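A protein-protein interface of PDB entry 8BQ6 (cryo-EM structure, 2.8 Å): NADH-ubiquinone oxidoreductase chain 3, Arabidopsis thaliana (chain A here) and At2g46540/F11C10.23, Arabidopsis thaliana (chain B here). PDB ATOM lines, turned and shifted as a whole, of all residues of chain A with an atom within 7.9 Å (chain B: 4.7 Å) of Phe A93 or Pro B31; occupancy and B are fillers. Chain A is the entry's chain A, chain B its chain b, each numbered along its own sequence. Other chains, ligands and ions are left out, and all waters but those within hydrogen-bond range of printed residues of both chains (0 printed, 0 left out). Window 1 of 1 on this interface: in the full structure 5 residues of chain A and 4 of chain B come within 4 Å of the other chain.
Printed residues of chain B within 4 Å of Phe A93: Pro B31 (3.5 Å).
Pro B31 touches just one residue of chain A: Phe A93.
Of chain A, only Trp A94 comes within 4 Å of Ala B32.
Of the printed residues of chain A, Leu B28 touches Trp A94 (3.8 Å) and Met A97 (3.7 Å).
Of the printed residues of chain B, Leu A90 touches Arg B35.
The nearest residue of chain B that does not touch Phe A93 is Gly B27 (4.1 Å).
The nearest residue of chain A that does not touch Pro B31 is Trp A94 (4.1 Å).
Leu A90 touches Arg B35 (CD1 to CG, 3.8 Å).
CG of Pro B31 touches CE2 of Phe A93 (3.5 Å).
CH2 of Trp A94 touches O of Leu B28, at 3.8 Å.
Ala B32 touches Trp A94.
SD of Met A97 touches CD2 of Leu B28, 3.7 Å away.
O of Leu B30 is in hydrogen-bond range of N of Arg B35, 3.0 Å away.
The side-chain carboxylate of Asp A89 is in salt-bridge range of the guanidinium group of Arg B35 (3.5 Å).
Printed residues of chain B that touch a printed residue of chain A: Leu B28, Pro B31, Ala B32 and Arg B35.
Hydrophobic or aromatic side chains of chain A within 4 Å of the printed part of chain B: Leu A90, Phe A93, Trp A94 and Met A97.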
ATOM      1  N   TRP A  81     -21.360  -3.785 -18.341  1.00  0.00           N
ATOM      2  CA  TRP A  81     -20.021  -3.210 -18.059  1.00  0.00           C
ATOM      3  C   TRP A  81     -18.932  -4.244 -18.336  1.00  0.00           C
ATOM      4  O   TRP A  81     -17.948  -3.888 -18.984  1.00  0.00           O
ATOM      5  CB  TRP A  81     -19.985  -2.722 -16.607  1.00  0.00           C
ATOM      6  CG  TRP A  81     -18.727  -2.028 -16.192  1.00  0.00           C
ATOM      7  CD1 TRP A  81     -18.333  -0.769 -16.531  1.00  0.00           C
ATOM      8  CD2 TRP A  81     -17.715  -2.547 -15.315  1.00  0.00           C
ATOM      9  NE1 TRP A  81     -17.134  -0.475 -15.944  1.00  0.00           N
ATOM     10  CE2 TRP A  81     -16.732  -1.544 -15.188  1.00  0.00           C
ATOM     11  CE3 TRP A  81     -17.540  -3.755 -14.633  1.00  0.00           C
ATOM     12  CZ2 TRP A  81     -15.593  -1.714 -14.404  1.00  0.00           C
ATOM     13  CZ3 TRP A  81     -16.414  -3.921 -13.858  1.00  0.00           C
ATOM     14  CH2 TRP A  81     -15.457  -2.914 -13.748  1.00  0.00           C
ATOM     15  N   SER A  84     -18.461  -4.734 -21.913  1.00  0.00           N
ATOM     16  CA  SER A  84     -18.089  -3.520 -22.629  1.00  0.00           C
ATOM     17  C   SER A  84     -16.788  -2.897 -22.150  1.00  0.00           C
ATOM     18  O   SER A  84     -16.421  -1.824 -22.637  1.00  0.00           O
ATOM     19  CB  SER A  84     -19.204  -2.478 -22.516  1.00  0.00           C
ATOM     20  OG  SER A  84     -20.477  -3.092 -22.543  1.00  0.00           O
ATOM     21  N   LEU A  85     -16.090  -3.536 -21.209  1.00  0.00           N
ATOM     22  CA  LEU A  85     -14.897  -2.926 -20.628  1.00  0.00           C
ATOM     23  C   LEU A  85     -13.848  -2.579 -21.680  1.00  0.00           C
ATOM     24  O   LEU A  85     -13.157  -1.563 -21.548  1.00  0.00           O
ATOM     25  CB  LEU A  85     -14.306  -3.861 -19.574  1.00  0.00           C
ATOM     26  CG  LEU A  85     -14.633  -3.577 -18.108  1.00  0.00           C
ATOM     27  CD1 LEU A  85     -13.943  -4.602 -17.235  1.00  0.00           C
ATOM     28  CD2 LEU A  85     -14.218  -2.173 -17.707  1.00  0.00           C
ATOM     29  N   ILE A  88     -15.099   0.924 -23.258  1.00  0.00           N
ATOM     30  CA  ILE A  88     -15.284   2.093 -22.404  1.00  0.00           C
ATOM     31  C   ILE A  88     -13.996   2.534 -21.721  1.00  0.00           C
ATOM     32  O   ILE A  88     -13.896   3.695 -21.307  1.00  0.00           O
ATOM     33  CB  ILE A  88     -16.368   1.827 -21.349  1.00  0.00           C
ATOM     34  CG1 ILE A  88     -15.986   0.623 -20.488  1.00  0.00           C
ATOM     35  CG2 ILE A  88     -17.705   1.600 -22.025  1.00  0.00           C
ATOM     36  CD1 ILE A  88     -17.060   0.191 -19.539  1.00  0.00           C
ATOM     37  N   ASP A  89     -13.030   1.637 -21.563  1.00  0.00           N
ATOM     38  CA  ASP A  89     -11.658   1.968 -21.132  1.00  0.00           C
ATOM     39  C   ASP A  89     -11.699   2.541 -19.709  1.00  0.00           C
ATOM     40  O   ASP A  89     -12.380   1.984 -18.836  1.00  0.00           O
ATOM     41  CB  ASP A  89     -11.013   2.873 -22.151  1.00  0.00           C
ATOM     42  CG  ASP A  89      -9.511   2.936 -21.995  1.00  0.00           C
ATOM     43  OD1 ASP A  89      -8.961   2.114 -21.233  1.00  0.00           O
ATOM     44  OD2 ASP A  89      -8.884   3.821 -22.609  1.00  0.00           O
ATOM     45  N   LEU A  90     -10.979   3.635 -19.447  1.00  0.00           N
ATOM     46  CA  LEU A  90     -10.804   4.110 -18.078  1.00  0.00           C
ATOM     47  C   LEU A  90     -12.007   4.905 -17.597  1.00  0.00           C
ATOM     48  O   LEU A  90     -12.355   4.854 -16.411  1.00  0.00           O
ATOM     49  CB  LEU A  90      -9.538   4.954 -17.979  1.00  0.00           C
ATOM     50  CG  LEU A  90      -8.270   4.130 -17.792  1.00  0.00           C
ATOM     51  CD1 LEU A  90      -7.056   5.031 -17.811  1.00  0.00           C
ATOM     52  CD2 LEU A  90      -8.347   3.357 -16.493  1.00  0.00           C
ATOM     53  N   PHE A  91     -12.608   5.694 -18.485  1.00  0.00           N
ATOM     54  CA  PHE A  91     -13.813   6.469 -18.105  1.00  0.00           C
ATOM     55  C   PHE A  91     -14.887   5.506 -17.583  1.00  0.00           C
ATOM     56  O   PHE A  91     -15.408   5.763 -16.490  1.00  0.00           O
ATOM     57  CB  PHE A  91     -14.309   7.339 -19.263  1.00  0.00           C
ATOM     58  CG  PHE A  91     -15.206   8.479 -18.860  1.00  0.00           C
ATOM     59  CD1 PHE A  91     -16.545   8.267 -18.580  1.00  0.00           C
ATOM     60  CD2 PHE A  91     -14.707   9.768 -18.761  1.00  0.00           C
ATOM     61  CE1 PHE A  91     -17.365   9.318 -18.206  1.00  0.00           C
ATOM     62  CE2 PHE A  91     -15.529  10.820 -18.392  1.00  0.00           C
ATOM     63  CZ  PHE A  91     -16.855  10.592 -18.114  1.00  0.00           C
ATOM     64  N   GLY A  92     -15.195   4.440 -18.328  1.00  0.00           N
ATOM     65  CA  GLY A  92     -16.223   3.507 -17.895  1.00  0.00           C
ATOM     66  C   GLY A  92     -15.866   2.812 -16.596  1.00  0.00           C
ATOM     67  O   GLY A  92     -16.723   2.615 -15.722  1.00  0.00           O
ATOM     68  N   PHE A  93     -14.591   2.449 -16.443  1.00  0.00           N
ATOM     69  CA  PHE A  93     -14.141   1.812 -15.214  1.00  0.00           C
ATOM     70  C   PHE A  93     -14.405   2.703 -14.007  1.00  0.00           C
ATOM     71  O   PHE A  93     -14.948   2.252 -12.992  1.00  0.00           O
ATOM     72  CB  PHE A  93     -12.654   1.475 -15.321  1.00  0.00           C
ATOM     73  CG  PHE A  93     -12.066   0.963 -14.047  1.00  0.00           C
ATOM     74  CD1 PHE A  93     -12.177  -0.370 -13.710  1.00  0.00           C
ATOM     75  CD2 PHE A  93     -11.424   1.819 -13.173  1.00  0.00           C
ATOM     76  CE1 PHE A  93     -11.649  -0.840 -12.533  1.00  0.00           C
ATOM     77  CE2 PHE A  93     -10.894   1.350 -11.994  1.00  0.00           C
ATOM     78  CZ  PHE A  93     -11.007   0.020 -11.676  1.00  0.00           C
ATOM     79  N   TRP A  94     -14.050   3.986 -14.107  1.00  0.00           N
ATOM     80  CA  TRP A  94     -14.174   4.869 -12.954  1.00  0.00           C
ATOM     81  C   TRP A  94     -15.622   5.249 -12.671  1.00  0.00           C
ATOM     82  O   TRP A  94     -15.983   5.457 -11.508  1.00  0.00           O
ATOM     83  CB  TRP A  94     -13.306   6.110 -13.149  1.00  0.00           C
ATOM     84  CG  TRP A  94     -11.869   5.796 -12.932  1.00  0.00           C
ATOM     85  CD1 TRP A  94     -10.866   5.891 -13.845  1.00  0.00           C
ATOM     86  CD2 TRP A  94     -11.273   5.300 -11.728  1.00  0.00           C
ATOM     87  NE1 TRP A  94      -9.678   5.492 -13.285  1.00  0.00           N
ATOM     88  CE2 TRP A  94      -9.901   5.126 -11.985  1.00  0.00           C
ATOM     89  CE3 TRP A  94     -11.765   4.994 -10.457  1.00  0.00           C
ATOM     90  CZ2 TRP A  94      -9.016   4.662 -11.020  1.00  0.00           C
ATOM     91  CZ3 TRP A  94     -10.885   4.534  -9.501  1.00  0.00           C
ATOM     92  CH2 TRP A  94      -9.526   4.370  -9.788  1.00  0.00           C
ATOM     93  N   SER A  95     -16.471   5.332 -13.699  1.00  0.00           N
ATOM     94  CA  SER A  95     -17.885   5.581 -13.432  1.00  0.00           C
ATOM     95  C   SER A  95     -18.518   4.392 -12.717  1.00  0.00           C
ATOM     96  O   SER A  95     -19.322   4.566 -11.787  1.00  0.00           O
ATOM     97  CB  SER A  95     -18.634   5.908 -14.725  1.00  0.00           C
ATOM     98  OG  SER A  95     -18.620   4.823 -15.633  1.00  0.00           O
ATOM     99  N   MET A  96     -18.132   3.176 -13.104  1.00  0.00           N
ATOM    100  CA  MET A  96     -18.626   1.984 -12.362  1.00  0.00           C
ATOM    101  C   MET A  96     -18.063   1.991 -10.935  1.00  0.00           C
ATOM    102  O   MET A  96     -18.808   1.647 -10.014  1.00  0.00           O
ATOM    103  CB  MET A  96     -18.233   0.673 -13.042  1.00  0.00           C
ATOM    104  CG  MET A  96     -18.643  -0.569 -12.267  1.00  0.00           C
ATOM    105  SD  MET A  96     -20.409  -0.658 -11.873  1.00  0.00           S
ATOM    106  CE  MET A  96     -21.080  -1.188 -13.446  1.00  0.00           C
ATOM    107  N   MET A  97     -16.809   2.400 -10.761  1.00  0.00           N
ATOM    108  CA  MET A  97     -16.246   2.462  -9.413  1.00  0.00           C
ATOM    109  C   MET A  97     -17.004   3.453  -8.539  1.00  0.00           C
ATOM    110  O   MET A  97     -17.234   3.194  -7.354  1.00  0.00           O
ATOM    111  CB  MET A  97     -14.765   2.827  -9.470  1.00  0.00           C
ATOM    112  CG  MET A  97     -13.869   1.699  -9.928  1.00  0.00           C
ATOM    113  SD  MET A  97     -14.228   0.143  -9.096  1.00  0.00           S
ATOM    114  CE  MET A  97     -14.874  -0.819 -10.455  1.00  0.00           C
ATOM    115  N   ALA A  98     -17.386   4.602  -9.097  1.00  0.00           N
ATOM    116  CA  ALA A  98     -18.179   5.557  -8.327  1.00  0.00           C
ATOM    117  C   ALA A  98     -19.535   4.967  -7.948  1.00  0.00           C
ATOM    118  O   ALA A  98     -20.001   5.121  -6.806  1.00  0.00           O
ATOM    119  CB  ALA A  98     -18.347   6.851  -9.121  1.00  0.00           C
ATOM    120  N   PHE A  99     -20.180   4.285  -8.899  1.00  0.00           N
ATOM    121  CA  PHE A  99     -21.429   3.583  -8.616  1.00  0.00           C
ATOM    122  C   PHE A  99     -21.270   2.610  -7.448  1.00  0.00           C
ATOM    123  O   PHE A  99     -22.063   2.610  -6.489  1.00  0.00           O
ATOM    124  CB  PHE A  99     -21.869   2.856  -9.888  1.00  0.00           C
ATOM    125  CG  PHE A  99     -23.198   2.187  -9.788  1.00  0.00           C
ATOM    126  CD1 PHE A  99     -24.354   2.874 -10.104  1.00  0.00           C
ATOM    127  CD2 PHE A  99     -23.290   0.855  -9.433  1.00  0.00           C
ATOM    128  CE1 PHE A  99     -25.581   2.255 -10.034  1.00  0.00           C
ATOM    129  CE2 PHE A  99     -24.512   0.231  -9.362  1.00  0.00           C
ATOM    130  CZ  PHE A  99     -25.660   0.931  -9.660  1.00  0.00           C
ATOM    131  N   LEU A 100     -20.240   1.773  -7.528  1.00  0.00           N
ATOM    132  CA  LEU A 100     -19.979   0.794  -6.449  1.00  0.00           C
ATOM    133  C   LEU A 100     -19.746   1.540  -5.138  1.00  0.00           C
ATOM    134  O   LEU A 100     -20.259   1.082  -4.121  1.00  0.00           O
ATOM    135  CB  LEU A 100     -18.756  -0.041  -6.830  1.00  0.00           C
ATOM    136  CG  LEU A 100     -18.989  -1.040  -7.958  1.00  0.00           C
ATOM    137  CD1 LEU A 100     -17.709  -1.786  -8.290  1.00  0.00           C
ATOM    138  CD2 LEU A 100     -20.094  -2.009  -7.582  1.00  0.00           C
ATOM    139  N   VAL B  26      -5.889  -3.059  -4.117  1.00  0.00           N
ATOM    140  CA  VAL B  26      -4.967  -3.286  -5.228  1.00  0.00           C
ATOM    141  C   VAL B  26      -5.685  -3.068  -6.553  1.00  0.00           C
ATOM    142  O   VAL B  26      -5.143  -2.445  -7.482  1.00  0.00           O
ATOM    143  CB  VAL B  26      -4.348  -4.692  -5.140  1.00  0.00           C
ATOM    144  CG1 VAL B  26      -3.915  -5.168  -6.513  1.00  0.00           C
ATOM    145  CG2 VAL B  26      -3.167  -4.683  -4.190  1.00  0.00           C
ATOM    146  N   GLY B  27      -6.924  -3.565  -6.654  1.00  0.00           N
ATOM    147  CA  GLY B  27      -7.706  -3.340  -7.860  1.00  0.00           C
ATOM    148  C   GLY B  27      -7.937  -1.875  -8.184  1.00  0.00           C
ATOM    149  O   GLY B  27      -8.022  -1.502  -9.354  1.00  0.00           O
ATOM    150  N   LEU B  28      -8.090  -1.035  -7.163  1.00  0.00           N
ATOM    151  CA  LEU B  28      -8.239   0.401  -7.389  1.00  0.00           C
ATOM    152  C   LEU B  28      -6.905   1.100  -7.606  1.00  0.00           C
ATOM    153  O   LEU B  28      -6.814   2.042  -8.399  1.00  0.00           O
ATOM    154  CB  LEU B  28      -8.957   1.056  -6.212  1.00  0.00           C
ATOM    155  CG  LEU B  28     -10.416   0.680  -5.996  1.00  0.00           C
ATOM    156  CD1 LEU B  28     -10.919   1.345  -4.735  1.00  0.00           C
ATOM    157  CD2 LEU B  28     -11.246   1.095  -7.196  1.00  0.00           C
ATOM    158  N   PHE B  29      -5.874   0.655  -6.892  1.00  0.00           N
ATOM    159  CA  PHE B  29      -4.568   1.290  -6.959  1.00  0.00           C
ATOM    160  C   PHE B  29      -3.946   1.130  -8.337  1.00  0.00           C
ATOM    161  O   PHE B  29      -3.361   2.079  -8.871  1.00  0.00           O
ATOM    162  CB  PHE B  29      -3.671   0.697  -5.872  1.00  0.00           C
ATOM    163  CG  PHE B  29      -2.258   1.187  -5.913  1.00  0.00           C
ATOM    164  CD1 PHE B  29      -1.873   2.297  -5.182  1.00  0.00           C
ATOM    165  CD2 PHE B  29      -1.310   0.537  -6.685  1.00  0.00           C
ATOM    166  CE1 PHE B  29      -0.569   2.744  -5.221  1.00  0.00           C
ATOM    167  CE2 PHE B  29      -0.012   0.986  -6.733  1.00  0.00           C
ATOM    168  CZ  PHE B  29       0.361   2.089  -5.999  1.00  0.00           C
ATOM    169  N   LEU B  30      -4.056  -0.061  -8.932  1.00  0.00           N
ATOM    170  CA  LEU B  30      -3.390  -0.282 -10.215  1.00  0.00           C
ATOM    171  C   LEU B  30      -3.831   0.696 -11.298  1.00  0.00           C
ATOM    172  O   LEU B  30      -2.959   1.361 -11.884  1.00  0.00           O
ATOM    173  CB  LEU B  30      -3.584  -1.732 -10.663  1.00  0.00           C
ATOM    174  CG  LEU B  30      -2.633  -2.751 -10.058  1.00  0.00           C
ATOM    175  CD1 LEU B  30      -3.286  -4.105 -10.133  1.00  0.00           C
ATOM    176  CD2 LEU B  30      -1.308  -2.733 -10.795  1.00  0.00           C
ATOM    177  N   PRO B  31      -5.124   0.857 -11.610  1.00  0.00           N
ATOM    178  CA  PRO B  31      -5.490   1.839 -12.641  1.00  0.00           C
ATOM    179  C   PRO B  31      -5.229   3.274 -12.229  1.00  0.00           C
ATOM    180  O   PRO B  31      -4.965   4.114 -13.097  1.00  0.00           O
ATOM    181  CB  PRO B  31      -6.987   1.585 -12.855  1.00  0.00           C
ATOM    182  CG  PRO B  31      -7.432   0.901 -11.637  1.00  0.00           C
ATOM    183  CD  PRO B  31      -6.293   0.067 -11.197  1.00  0.00           C
ATOM    184  N   ALA B  32      -5.313   3.584 -10.936  1.00  0.00           N
ATOM    185  CA  ALA B  32      -5.140   4.963 -10.493  1.00  0.00           C
ATOM    186  C   ALA B  32      -3.693   5.414 -10.621  1.00  0.00           C
ATOM    187  O   ALA B  32      -3.422   6.529 -11.081  1.00  0.00           O
ATOM    188  CB  ALA B  32      -5.615   5.112  -9.051  1.00  0.00           C
ATOM    189  N   VAL B  33      -2.752   4.570 -10.217  1.00  0.00           N
ATOM    190  CA  VAL B  33      -1.345   4.937 -10.138  1.00  0.00           C
ATOM    191  C   VAL B  33      -0.532   4.285 -11.247  1.00  0.00           C
ATOM    192  O   VAL B  33       0.157   4.969 -12.004  1.00  0.00           O
ATOM    193  CB  VAL B  33      -0.764   4.592  -8.748  1.00  0.00           C
ATOM    194  CG1 VAL B  33       0.737   4.795  -8.740  1.00  0.00           C
ATOM    195  CG2 VAL B  33      -1.414   5.454  -7.688  1.00  0.00           C
ATOM    196  N   ARG B  35      -1.354   2.665 -14.046  1.00  0.00           N
ATOM    197  CA  ARG B  35      -1.753   2.852 -15.438  1.00  0.00           C
ATOM    198  C   ARG B  35      -1.267   4.176 -16.021  1.00  0.00           C
ATOM    199  O   ARG B  35      -0.717   4.164 -17.137  1.00  0.00           O
ATOM    200  CB  ARG B  35      -3.270   2.670 -15.554  1.00  0.00           C
ATOM    201  CG  ARG B  35      -3.863   3.194 -16.829  1.00  0.00           C
ATOM    202  CD  ARG B  35      -3.542   2.300 -18.004  1.00  0.00           C
ATOM    203  NE  ARG B  35      -4.105   2.865 -19.222  1.00  0.00           N
ATOM    204  CZ  ARG B  35      -5.129   2.349 -19.887  1.00  0.00           C
ATOM    205  NH1 ARG B  35      -5.689   1.210 -19.516  1.00  0.00           N
ATOM    206  NH2 ARG B  35      -5.598   2.991 -20.952  1.00  0.00           N
ATOM    207  N   PRO B  36      -1.410   5.376 -15.378  1.00  0.00           N
ATOM    208  CA  PRO B  36      -0.787   6.596 -15.911  1.00  0.00           C
ATOM    209  C   PRO B  36       0.745   6.482 -16.012  1.00  0.00           C
ATOM    210  O   PRO B  36       1.284   7.088 -16.905  1.00  0.00           O
ATOM    211  CB  PRO B  36      -1.145   7.736 -14.949  1.00  0.00           C
ATOM    212  CG  PRO B  36      -1.678   7.059 -13.733  1.00  0.00           C
ATOM    213  CD  PRO B  36      -2.285   5.777 -14.250  1.00  0.00           C
